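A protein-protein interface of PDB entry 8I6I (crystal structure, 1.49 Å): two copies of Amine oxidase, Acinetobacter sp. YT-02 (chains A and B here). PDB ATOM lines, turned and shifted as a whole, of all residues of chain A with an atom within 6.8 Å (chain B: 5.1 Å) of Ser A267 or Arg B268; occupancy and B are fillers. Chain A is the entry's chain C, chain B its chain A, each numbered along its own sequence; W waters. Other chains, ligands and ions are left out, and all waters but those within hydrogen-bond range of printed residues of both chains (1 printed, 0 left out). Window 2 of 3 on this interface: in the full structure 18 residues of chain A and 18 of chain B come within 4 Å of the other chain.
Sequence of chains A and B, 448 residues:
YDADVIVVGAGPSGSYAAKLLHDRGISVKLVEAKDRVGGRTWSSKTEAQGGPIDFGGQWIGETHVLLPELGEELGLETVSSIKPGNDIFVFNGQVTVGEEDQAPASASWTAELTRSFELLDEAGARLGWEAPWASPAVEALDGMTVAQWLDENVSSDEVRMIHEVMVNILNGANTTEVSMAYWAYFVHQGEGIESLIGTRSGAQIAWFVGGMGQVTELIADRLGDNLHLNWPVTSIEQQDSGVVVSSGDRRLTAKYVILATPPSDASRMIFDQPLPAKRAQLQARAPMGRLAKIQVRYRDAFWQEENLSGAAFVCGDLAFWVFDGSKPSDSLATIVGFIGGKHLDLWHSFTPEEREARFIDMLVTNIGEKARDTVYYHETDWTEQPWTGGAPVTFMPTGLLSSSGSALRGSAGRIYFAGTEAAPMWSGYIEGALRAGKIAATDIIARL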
ATOM      1  N   THR A 234       2.594  31.932  -4.114  1.00  0.00           N
ATOM      2  CA  THR A 234       2.501  31.539  -2.691  1.00  0.00           C
ATOM      3  C   THR A 234       1.687  32.533  -1.883  1.00  0.00           C
ATOM      4  O   THR A 234       1.149  32.121  -0.844  1.00  0.00           O
ATOM      5  CB  THR A 234       3.906  31.319  -2.119  1.00  0.00           C
ATOM      6  OG1 THR A 234       4.677  32.507  -2.344  1.00  0.00           O
ATOM      7  CG2 THR A 234       4.551  30.143  -2.802  1.00  0.00           C
ATOM      8  N   THR A 261      -7.375  30.046 -11.602  1.00  0.00           N
ATOM      9  CA  THR A 261      -7.112  28.695 -11.081  1.00  0.00           C
ATOM     10  C   THR A 261      -8.411  28.164 -10.506  1.00  0.00           C
ATOM     11  O   THR A 261      -9.336  28.910 -10.176  1.00  0.00           O
ATOM     12  CB  THR A 261      -5.979  28.656 -10.055  1.00  0.00           C
ATOM     13  OG1 THR A 261      -6.445  29.126  -8.791  1.00  0.00           O
ATOM     14  CG2 THR A 261      -4.758  29.427 -10.454  1.00  0.00           C
ATOM     15  N   PRO A 262      -8.526  26.839 -10.345  1.00  0.00           N
ATOM     16  CA  PRO A 262      -9.651  26.289  -9.622  1.00  0.00           C
ATOM     17  C   PRO A 262      -9.664  26.796  -8.191  1.00  0.00           C
ATOM     18  O   PRO A 262      -8.625  27.129  -7.634  1.00  0.00           O
ATOM     19  CB  PRO A 262      -9.433  24.790  -9.614  1.00  0.00           C
ATOM     20  CG  PRO A 262      -8.374  24.516 -10.598  1.00  0.00           C
ATOM     21  CD  PRO A 262      -7.693  25.805 -10.970  1.00  0.00           C
ATOM     22  N   PRO A 263     -10.832  26.880  -7.560  1.00  0.00           N
ATOM     23  CA  PRO A 263     -10.905  27.323  -6.171  1.00  0.00           C
ATOM     24  C   PRO A 263      -9.976  26.537  -5.241  1.00  0.00           C
ATOM     25  O   PRO A 263      -9.308  27.137  -4.403  1.00  0.00           O
ATOM     26  CB  PRO A 263     -12.387  27.057  -5.834  1.00  0.00           C
ATOM     27  CG  PRO A 263     -13.105  27.285  -7.161  1.00  0.00           C
ATOM     28  CD  PRO A 263     -12.162  26.611  -8.136  1.00  0.00           C
ATOM     29  N   SER A 264      -9.910  25.210  -5.421  1.00  0.00           N
ATOM     30  CA  SER A 264      -9.066  24.389  -4.557  1.00  0.00           C
ATOM     31  C   SER A 264      -7.577  24.753  -4.736  1.00  0.00           C
ATOM     32  O   SER A 264      -6.802  24.749  -3.754  1.00  0.00           O
ATOM     33  CB  SER A 264      -9.361  22.931  -4.803  1.00  0.00           C
ATOM     34  OG  SER A 264      -9.018  22.652  -6.138  1.00  0.00           O
ATOM     35  N   ASP A 265      -7.114  25.050  -5.922  1.00  0.00           N
ATOM     36  CA  ASP A 265      -5.692  25.462  -6.110  1.00  0.00           C
ATOM     37  C   ASP A 265      -5.478  26.883  -5.587  1.00  0.00           C
ATOM     38  O   ASP A 265      -4.367  27.198  -5.059  1.00  0.00           O
ATOM     39  CB  ASP A 265      -5.285  25.106  -7.533  1.00  0.00           C
ATOM     40  CG  ASP A 265      -5.219  23.560  -7.654  1.00  0.00           C
ATOM     41  OD1 ASP A 265      -4.599  22.860  -6.760  1.00  0.00           O
ATOM     42  OD2 ASP A 265      -5.870  23.006  -8.554  1.00  0.00           O
ATOM     43  N   ALA A 266      -6.484  27.745  -5.592  1.00  0.00           N
ATOM     44  CA  ALA A 266      -6.402  29.087  -4.986  1.00  0.00           C
ATOM     45  C   ALA A 266      -6.236  28.973  -3.476  1.00  0.00           C
ATOM     46  O   ALA A 266      -5.566  29.798  -2.890  1.00  0.00           O
ATOM     47  CB  ALA A 266      -7.614  29.902  -5.337  1.00  0.00           C
ATOM     48  N   SER A 267      -6.771  27.927  -2.862  1.00  0.00           N
ATOM     49  CA  SER A 267      -6.664  27.763  -1.400  1.00  0.00           C
ATOM     50  C   SER A 267      -5.207  27.617  -0.983  1.00  0.00           C
ATOM     51  O   SER A 267      -4.915  27.851   0.210  1.00  0.00           O
ATOM     52  CB  SER A 267      -7.501  26.607  -0.874  1.00  0.00           C
ATOM     53  OG  SER A 267      -6.880  25.367  -1.202  1.00  0.00           O
ATOM     54  N   ARG A 268      -4.307  27.122  -1.823  1.00  0.00           N
ATOM     55  CA  ARG A 268      -2.881  26.952  -1.486  1.00  0.00           C
ATOM     56  C   ARG A 268      -2.293  28.324  -1.232  1.00  0.00           C
ATOM     57  O   ARG A 268      -1.364  28.410  -0.447  1.00  0.00           O
ATOM     58  CB  ARG A 268      -2.207  26.238  -2.675  1.00  0.00           C
ATOM     59  CG  ARG A 268      -0.720  25.979  -2.562  1.00  0.00           C
ATOM     60  CD  ARG A 268      -0.275  25.158  -3.728  1.00  0.00           C
ATOM     61  NE  ARG A 268      -0.635  23.758  -3.536  1.00  0.00           N
ATOM     62  CZ  ARG A 268      -1.471  23.045  -4.297  1.00  0.00           C
ATOM     63  NH1 ARG A 268      -2.024  23.529  -5.400  1.00  0.00           N
ATOM     64  NH2 ARG A 268      -1.689  21.780  -4.006  1.00  0.00           N
ATOM     65  N   MET A 269      -2.743  29.361  -1.924  1.00  0.00           N
ATOM     66  CA  MET A 269      -2.137  30.693  -1.833  1.00  0.00           C
ATOM     67  C   MET A 269      -2.556  31.347  -0.513  1.00  0.00           C
ATOM     68  O   MET A 269      -3.678  31.190  -0.077  1.00  0.00           O
ATOM     69  CB  MET A 269      -2.614  31.565  -3.007  1.00  0.00           C
ATOM     70  CG  MET A 269      -2.338  30.942  -4.332  1.00  0.00           C
ATOM     71  SD  MET A 269      -3.273  31.823  -5.626  1.00  0.00           S
ATOM     72  CE  MET A 269      -3.137  30.613  -6.945  1.00  0.00           C
ATOM     73  N   ILE A 270      -1.667  32.111   0.110  1.00  0.00           N
ATOM     74  CA  ILE A 270      -1.986  32.897   1.317  1.00  0.00           C
ATOM     75  C   ILE A 270      -2.456  34.279   0.900  1.00  0.00           C
ATOM     76  O   ILE A 270      -1.694  34.974   0.215  1.00  0.00           O
ATOM     77  CB  ILE A 270      -0.766  32.965   2.247  1.00  0.00           C
ATOM     78  CG1 ILE A 270      -0.295  31.554   2.598  1.00  0.00           C
ATOM     79  CG2 ILE A 270      -1.102  33.783   3.498  1.00  0.00           C
ATOM     80  CD1 ILE A 270      -1.314  30.738   3.397  1.00  0.00           C
ATOM     81  N   PHE A 271      -3.629  34.687   1.346  1.00  0.00           N
ATOM     82  CA  PHE A 271      -4.198  36.022   1.059  1.00  0.00           C
ATOM     83  C   PHE A 271      -3.999  36.908   2.280  1.00  0.00           C
ATOM     84  O   PHE A 271      -4.476  36.560   3.349  1.00  0.00           O
ATOM     85  CB  PHE A 271      -5.659  35.916   0.619  1.00  0.00           C
ATOM     86  CG  PHE A 271      -5.820  35.161  -0.690  1.00  0.00           C
ATOM     87  CD1 PHE A 271      -5.818  33.790  -0.720  1.00  0.00           C
ATOM     88  CD2 PHE A 271      -5.992  35.827  -1.889  1.00  0.00           C
ATOM     89  CE1 PHE A 271      -5.910  33.096  -1.924  1.00  0.00           C
ATOM     90  CE2 PHE A 271      -6.033  35.133  -3.095  1.00  0.00           C
ATOM     91  CZ  PHE A 271      -6.055  33.778  -3.101  1.00  0.00           C
ATOM     92  N   ALA A 280     -13.410  32.135   0.877  1.00  0.00           N
ATOM     93  CA  ALA A 280     -12.417  31.294   1.582  1.00  0.00           C
ATOM     94  C   ALA A 280     -12.989  29.896   1.835  1.00  0.00           C
ATOM     95  O   ALA A 280     -12.279  28.879   1.588  1.00  0.00           O
ATOM     96  CB  ALA A 280     -12.005  31.950   2.850  1.00  0.00           C
ATOM     97  N   LEU A 282     -15.421  28.433  -0.009  1.00  0.00           N
ATOM     98  CA  LEU A 282     -15.515  27.812  -1.329  1.00  0.00           C
ATOM     99  C   LEU A 282     -14.158  27.188  -1.705  1.00  0.00           C
ATOM    100  O   LEU A 282     -14.075  26.015  -2.164  1.00  0.00           O
ATOM    101  CB  LEU A 282     -15.925  28.884  -2.340  1.00  0.00           C
ATOM    102  CG  LEU A 282     -16.064  28.349  -3.747  1.00  0.00           C
ATOM    103  CD1 LEU A 282     -17.234  27.385  -3.879  1.00  0.00           C
ATOM    104  CD2 LEU A 282     -16.205  29.519  -4.719  1.00  0.00           C
ATOM    105  N   GLN A 283     -13.100  27.947  -1.586  1.00  0.00           N
ATOM    106  CA  GLN A 283     -11.749  27.473  -1.973  1.00  0.00           C
ATOM    107  C   GLN A 283     -11.357  26.260  -1.136  1.00  0.00           C
ATOM    108  O   GLN A 283     -10.711  25.343  -1.680  1.00  0.00           O
ATOM    109  CB  GLN A 283     -10.758  28.627  -1.846  1.00  0.00           C
ATOM    110  CG  GLN A 283     -11.019  29.775  -2.808  1.00  0.00           C
ATOM    111  CD  GLN A 283      -9.987  30.880  -2.843  1.00  0.00           C
ATOM    112  OE1 GLN A 283      -9.957  31.671  -3.790  1.00  0.00           O
ATOM    113  NE2 GLN A 283      -9.099  30.890  -1.872  1.00  0.00           N
ATOM    114  N   ALA A 284     -11.663  26.234   0.153  1.00  0.00           N
ATOM    115  CA  ALA A 284     -11.277  25.108   1.011  1.00  0.00           C
ATOM    116  C   ALA A 284     -12.102  23.844   0.781  1.00  0.00           C
ATOM    117  O   ALA A 284     -11.610  22.723   1.100  1.00  0.00           O
ATOM    118  CB  ALA A 284     -11.392  25.553   2.435  1.00  0.00           C
ATOM    119  N   ARG A 285     -13.316  24.006   0.281  1.00  0.00           N
ATOM    120  CA  ARG A 285     -14.315  22.915   0.397  1.00  0.00           C
ATOM    121  C   ARG A 285     -14.802  22.457  -0.958  1.00  0.00           C
ATOM    122  O   ARG A 285     -15.597  21.505  -0.938  1.00  0.00           O
ATOM    123  CB  ARG A 285     -15.449  23.311   1.358  1.00  0.00           C
ATOM    124  CG  ARG A 285     -14.956  23.320   2.809  1.00  0.00           C
ATOM    125  CD  ARG A 285     -15.932  24.028   3.761  1.00  0.00           C
ATOM    126  NE  ARG A 285     -17.332  23.615   3.667  1.00  0.00           N
ATOM    127  CZ  ARG A 285     -18.358  24.417   3.943  1.00  0.00           C
ATOM    128  NH1 ARG A 285     -19.593  23.971   3.773  1.00  0.00           N
ATOM    129  NH2 ARG A 285     -18.190  25.646   4.362  1.00  0.00           N
ATOM    130  N   TRP A 387       0.254  21.025  -8.795  1.00  0.00           N
ATOM    131  CA  TRP A 387      -0.539  22.296  -8.812  1.00  0.00           C
ATOM    132  C   TRP A 387      -1.831  22.148  -9.628  1.00  0.00           C
ATOM    133  O   TRP A 387      -2.394  23.144 -10.075  1.00  0.00           O
ATOM    134  CB  TRP A 387       0.248  23.495  -9.334  1.00  0.00           C
ATOM    135  CG  TRP A 387       1.401  23.895  -8.459  1.00  0.00           C
ATOM    136  CD1 TRP A 387       1.360  24.641  -7.312  1.00  0.00           C
ATOM    137  CD2 TRP A 387       2.773  23.603  -8.734  1.00  0.00           C
ATOM    138  NE1 TRP A 387       2.628  24.820  -6.842  1.00  0.00           N
ATOM    139  CE2 TRP A 387       3.497  24.156  -7.662  1.00  0.00           C
ATOM    140  CE3 TRP A 387       3.435  22.927  -9.753  1.00  0.00           C
ATOM    141  CZ2 TRP A 387       4.898  24.086  -7.622  1.00  0.00           C
ATOM    142  CZ3 TRP A 387       4.814  22.858  -9.713  1.00  0.00           C
ATOM    143  CH2 TRP A 387       5.521  23.390  -8.635  1.00  0.00           C
ATOM    144  N   THR B 234       6.907  24.483   1.220  1.00  0.00           N
ATOM    145  CA  THR B 234       6.279  24.571  -0.110  1.00  0.00           C
ATOM    146  C   THR B 234       6.441  23.246  -0.845  1.00  0.00           C
ATOM    147  O   THR B 234       5.576  22.951  -1.696  1.00  0.00           O
ATOM    148  CB  THR B 234       6.791  25.794  -0.859  1.00  0.00           C
ATOM    149  OG1 THR B 234       8.208  25.662  -0.937  1.00  0.00           O
ATOM    150  CG2 THR B 234       6.314  27.071  -0.221  1.00  0.00           C
ATOM    151  N   SER B 264      -5.551  19.062   5.492  1.00  0.00           N
ATOM    152  CA  SER B 264      -5.875  20.159   4.561  1.00  0.00           C
ATOM    153  C   SER B 264      -4.645  21.053   4.392  1.00  0.00           C
ATOM    154  O   SER B 264      -4.350  21.528   3.291  1.00  0.00           O
ATOM    155  CB  SER B 264      -7.074  20.916   5.016  1.00  0.00           C
ATOM    156  OG  SER B 264      -6.888  21.459   6.310  1.00  0.00           O
ATOM    157  N   ASP B 265      -3.924  21.310   5.443  1.00  0.00           N
ATOM    158  CA  ASP B 265      -2.729  22.196   5.349  1.00  0.00           C
ATOM    159  C   ASP B 265      -1.574  21.447   4.656  1.00  0.00           C
ATOM    160  O   ASP B 265      -0.823  22.071   3.902  1.00  0.00           O
ATOM    161  CB  ASP B 265      -2.458  22.874   6.698  1.00  0.00           C
ATOM    162  CG  ASP B 265      -3.570  23.926   6.963  1.00  0.00           C
ATOM    163  OD1 ASP B 265      -3.911  24.756   6.014  1.00  0.00           O
ATOM    164  OD2 ASP B 265      -4.187  23.905   8.040  1.00  0.00           O
ATOM    165  N   ALA B 266      -1.480  20.119   4.764  1.00  0.00           N
ATOM    166  CA  ALA B 266      -0.492  19.313   4.036  1.00  0.00           C
ATOM    167  C   ALA B 266      -0.782  19.375   2.544  1.00  0.00           C
ATOM    168  O   ALA B 266       0.160  19.316   1.741  1.00  0.00           O
ATOM    169  CB  ALA B 266      -0.479  17.915   4.583  1.00  0.00           C
ATOM    170  N   SER B 267      -2.052  19.536   2.146  1.00  0.00           N
ATOM    171  CA  SER B 267      -2.399  19.602   0.721  1.00  0.00           C
ATOM    172  C   SER B 267      -1.693  20.785   0.069  1.00  0.00           C
ATOM    173  O   SER B 267      -1.552  20.742  -1.162  1.00  0.00           O
ATOM    174  CB  SER B 267      -3.896  19.650   0.510  1.00  0.00           C
ATOM    175  OG  SER B 267      -4.381  20.958   0.727  1.00  0.00           O
ATOM    176  N   ARG B 268      -1.383  21.865   0.806  1.00  0.00           N
ATOM    177  CA  ARG B 268      -0.690  23.032   0.214  1.00  0.00           C
ATOM    178  C   ARG B 268       0.690  22.617  -0.304  1.00  0.00           C
ATOM    179  O   ARG B 268       1.209  23.212  -1.284  1.00  0.00           O
ATOM    180  CB  ARG B 268      -0.619  24.129   1.294  1.00  0.00           C
ATOM    181  CG  ARG B 268      -0.031  25.450   0.857  1.00  0.00           C
ATOM    182  CD  ARG B 268      -0.188  26.450   1.972  1.00  0.00           C
ATOM    183  NE  ARG B 268      -1.546  26.978   2.017  1.00  0.00           N
ATOM    184  CZ  ARG B 268      -2.443  26.873   2.995  1.00  0.00           C
ATOM    185  NH1 ARG B 268      -2.201  26.280   4.148  1.00  0.00           N
ATOM    186  NH2 ARG B 268      -3.627  27.425   2.834  1.00  0.00           N
ATOM    187  N   MET B 269       1.331  21.650   0.314  1.00  0.00           N
ATOM    188  CA  MET B 269       2.729  21.301  -0.030  1.00  0.00           C
ATOM    189  C   MET B 269       2.730  20.478  -1.302  1.00  0.00           C
ATOM    190  O   MET B 269       1.832  19.663  -1.495  1.00  0.00           O
ATOM    191  CB  MET B 269       3.355  20.486   1.096  1.00  0.00           C
ATOM    192  CG  MET B 269       3.270  21.202   2.425  1.00  0.00           C
ATOM    193  SD  MET B 269       3.641  20.096   3.800  1.00  0.00           S
ATOM    194  CE  MET B 269       3.004  21.043   5.177  1.00  0.00           C
ATOM    195  N   ILE B 270       3.713  20.673  -2.175  1.00  0.00           N
ATOM    196  CA  ILE B 270       3.907  19.793  -3.347  1.00  0.00           C
ATOM    197  C   ILE B 270       4.812  18.630  -2.996  1.00  0.00           C
ATOM    198  O   ILE B 270       5.954  18.838  -2.553  1.00  0.00           O
ATOM    199  CB  ILE B 270       4.458  20.614  -4.534  1.00  0.00           C
ATOM    200  CG1 ILE B 270       3.570  21.799  -4.878  1.00  0.00           C
ATOM    201  CG2 ILE B 270       4.701  19.700  -5.702  1.00  0.00           C
ATOM    202  CD1 ILE B 270       2.231  21.419  -5.417  1.00  0.00           C
ATOM    203  N   TRP B 387      -2.111  29.791   7.248  1.00  0.00           N
ATOM    204  CA  TRP B 387      -1.603  28.395   7.316  1.00  0.00           C
ATOM    205  C   TRP B 387      -2.303  27.600   8.436  1.00  0.00           C
ATOM    206  O   TRP B 387      -1.828  26.537   8.833  1.00  0.00           O
ATOM    207  CB  TRP B 387      -0.100  28.322   7.522  1.00  0.00           C
ATOM    208  CG  TRP B 387       0.717  28.894   6.419  1.00  0.00           C
ATOM    209  CD1 TRP B 387       1.056  28.308   5.232  1.00  0.00           C
ATOM    210  CD2 TRP B 387       1.375  30.174   6.460  1.00  0.00           C
ATOM    211  NE1 TRP B 387       1.878  29.158   4.531  1.00  0.00           N
ATOM    212  CE2 TRP B 387       2.042  30.310   5.237  1.00  0.00           C
ATOM    213  CE3 TRP B 387       1.439  31.200   7.401  1.00  0.00           C
ATOM    214  CZ2 TRP B 387       2.815  31.446   4.957  1.00  0.00           C
ATOM    215  CZ3 TRP B 387       2.186  32.332   7.109  1.00  0.00           C
ATOM    216  CH2 TRP B 387       2.827  32.458   5.889  1.00  0.00           C
HETATM  217  O   HOH W   1      -4.119  23.777  -0.494  1.00  0.00           O
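O of Ser A267 is in hydrogen-bond range of NH2 of Arg B268 (3.0 Å). The guanidinium group (NE) of Arg B268 is in hydrogen-bond range of the backbone carbonyl oxygen (O) of Arg A268 (2.9 Å). O of Ser B267 sits at hydrogen-bond distance from NH2 of Arg A268, 3.0 Å away.
The backbone carbonyl oxygen of Ser A264 sits at hydrogen-bond distance from the side-chain hydroxyl of Ser A267. N of Ile B270 lies within hydrogen-bond range of O of Thr B234 (3.0 Å). The guanidinium group (NH1) of Arg A268 is in salt-bridge range of the side-chain carboxylate (OD1) of Asp A265 (3.0 Å). OG of Ser B267 sits at hydrogen-bond distance from O of Ser B264. O of Thr A234 sits at hydrogen-bond distance from N of Ile A270 (3.0 Å). The side-chain carboxylate (OD1) of Asp B265 is in salt-bridge range of the guanidinium group (NH1) of Arg B268.
Trp B387 touches Ile A270 (NE1 to CD1, 3.7 Å). CE2 of Trp A387 touches CG1 of Ile B270, 3.6 Å away.
Printed residues of chain B within 4 Å of Ser A267: Arg B268. Of the printed residues of chain B, Ile A270 touches Trp B387. Printed residues of chain B within 4 Å of Trp A387: Ile B270 (3.6 Å). Of the printed residues of chain A, Arg B268 touches Ser A267 (3.0 Å) and Arg A268 (2.9 Å). Of the printed residues of chain A, Ile B270 touches Trp A387. The nearest printed residue of chain B that does not touch Ser A267 is Ser B267 (5.4 Å). The nearest printed residue of chain A that does not touch Arg B268 is Ile A270 (4.01 Å). The nearest printed residue of chain B that does not touch Arg A268 is Ile B270 (4.2 Å).
Hydrophobic or aromatic side chains of chain A that line the printed part of chain B: Ile A270 and Trp A387. Hydrophobic or aromatic side chains of chain B within 4 Å of the printed part of chain A: Ile B270 and Trp B387. Among the printed residues, 5 pairs touch across the chains. Among the printed residues, no Asp or Glu carboxylate lies within 4 Å of a Lys or Arg side-chain nitrogen of the other chain.
Ser A267 touches Arg B268, and with the chains exchanged Arg A268 touches Ser B267. Arg B268 touches its own counterpart, Arg A268. Ile A270 touches Trp B387, and with the chains exchanged Trp A387 touches Ile B270. 9 positions are printed for both chains. Of the 5 pairs that touch across the chains among the printed residues, 5 have their exchanged pair printed and touching as well.
Water W1 bridges the side-chain hydroxyl (OG) of Ser B267 and the side-chain hydroxyl (OG) of Ser A267.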
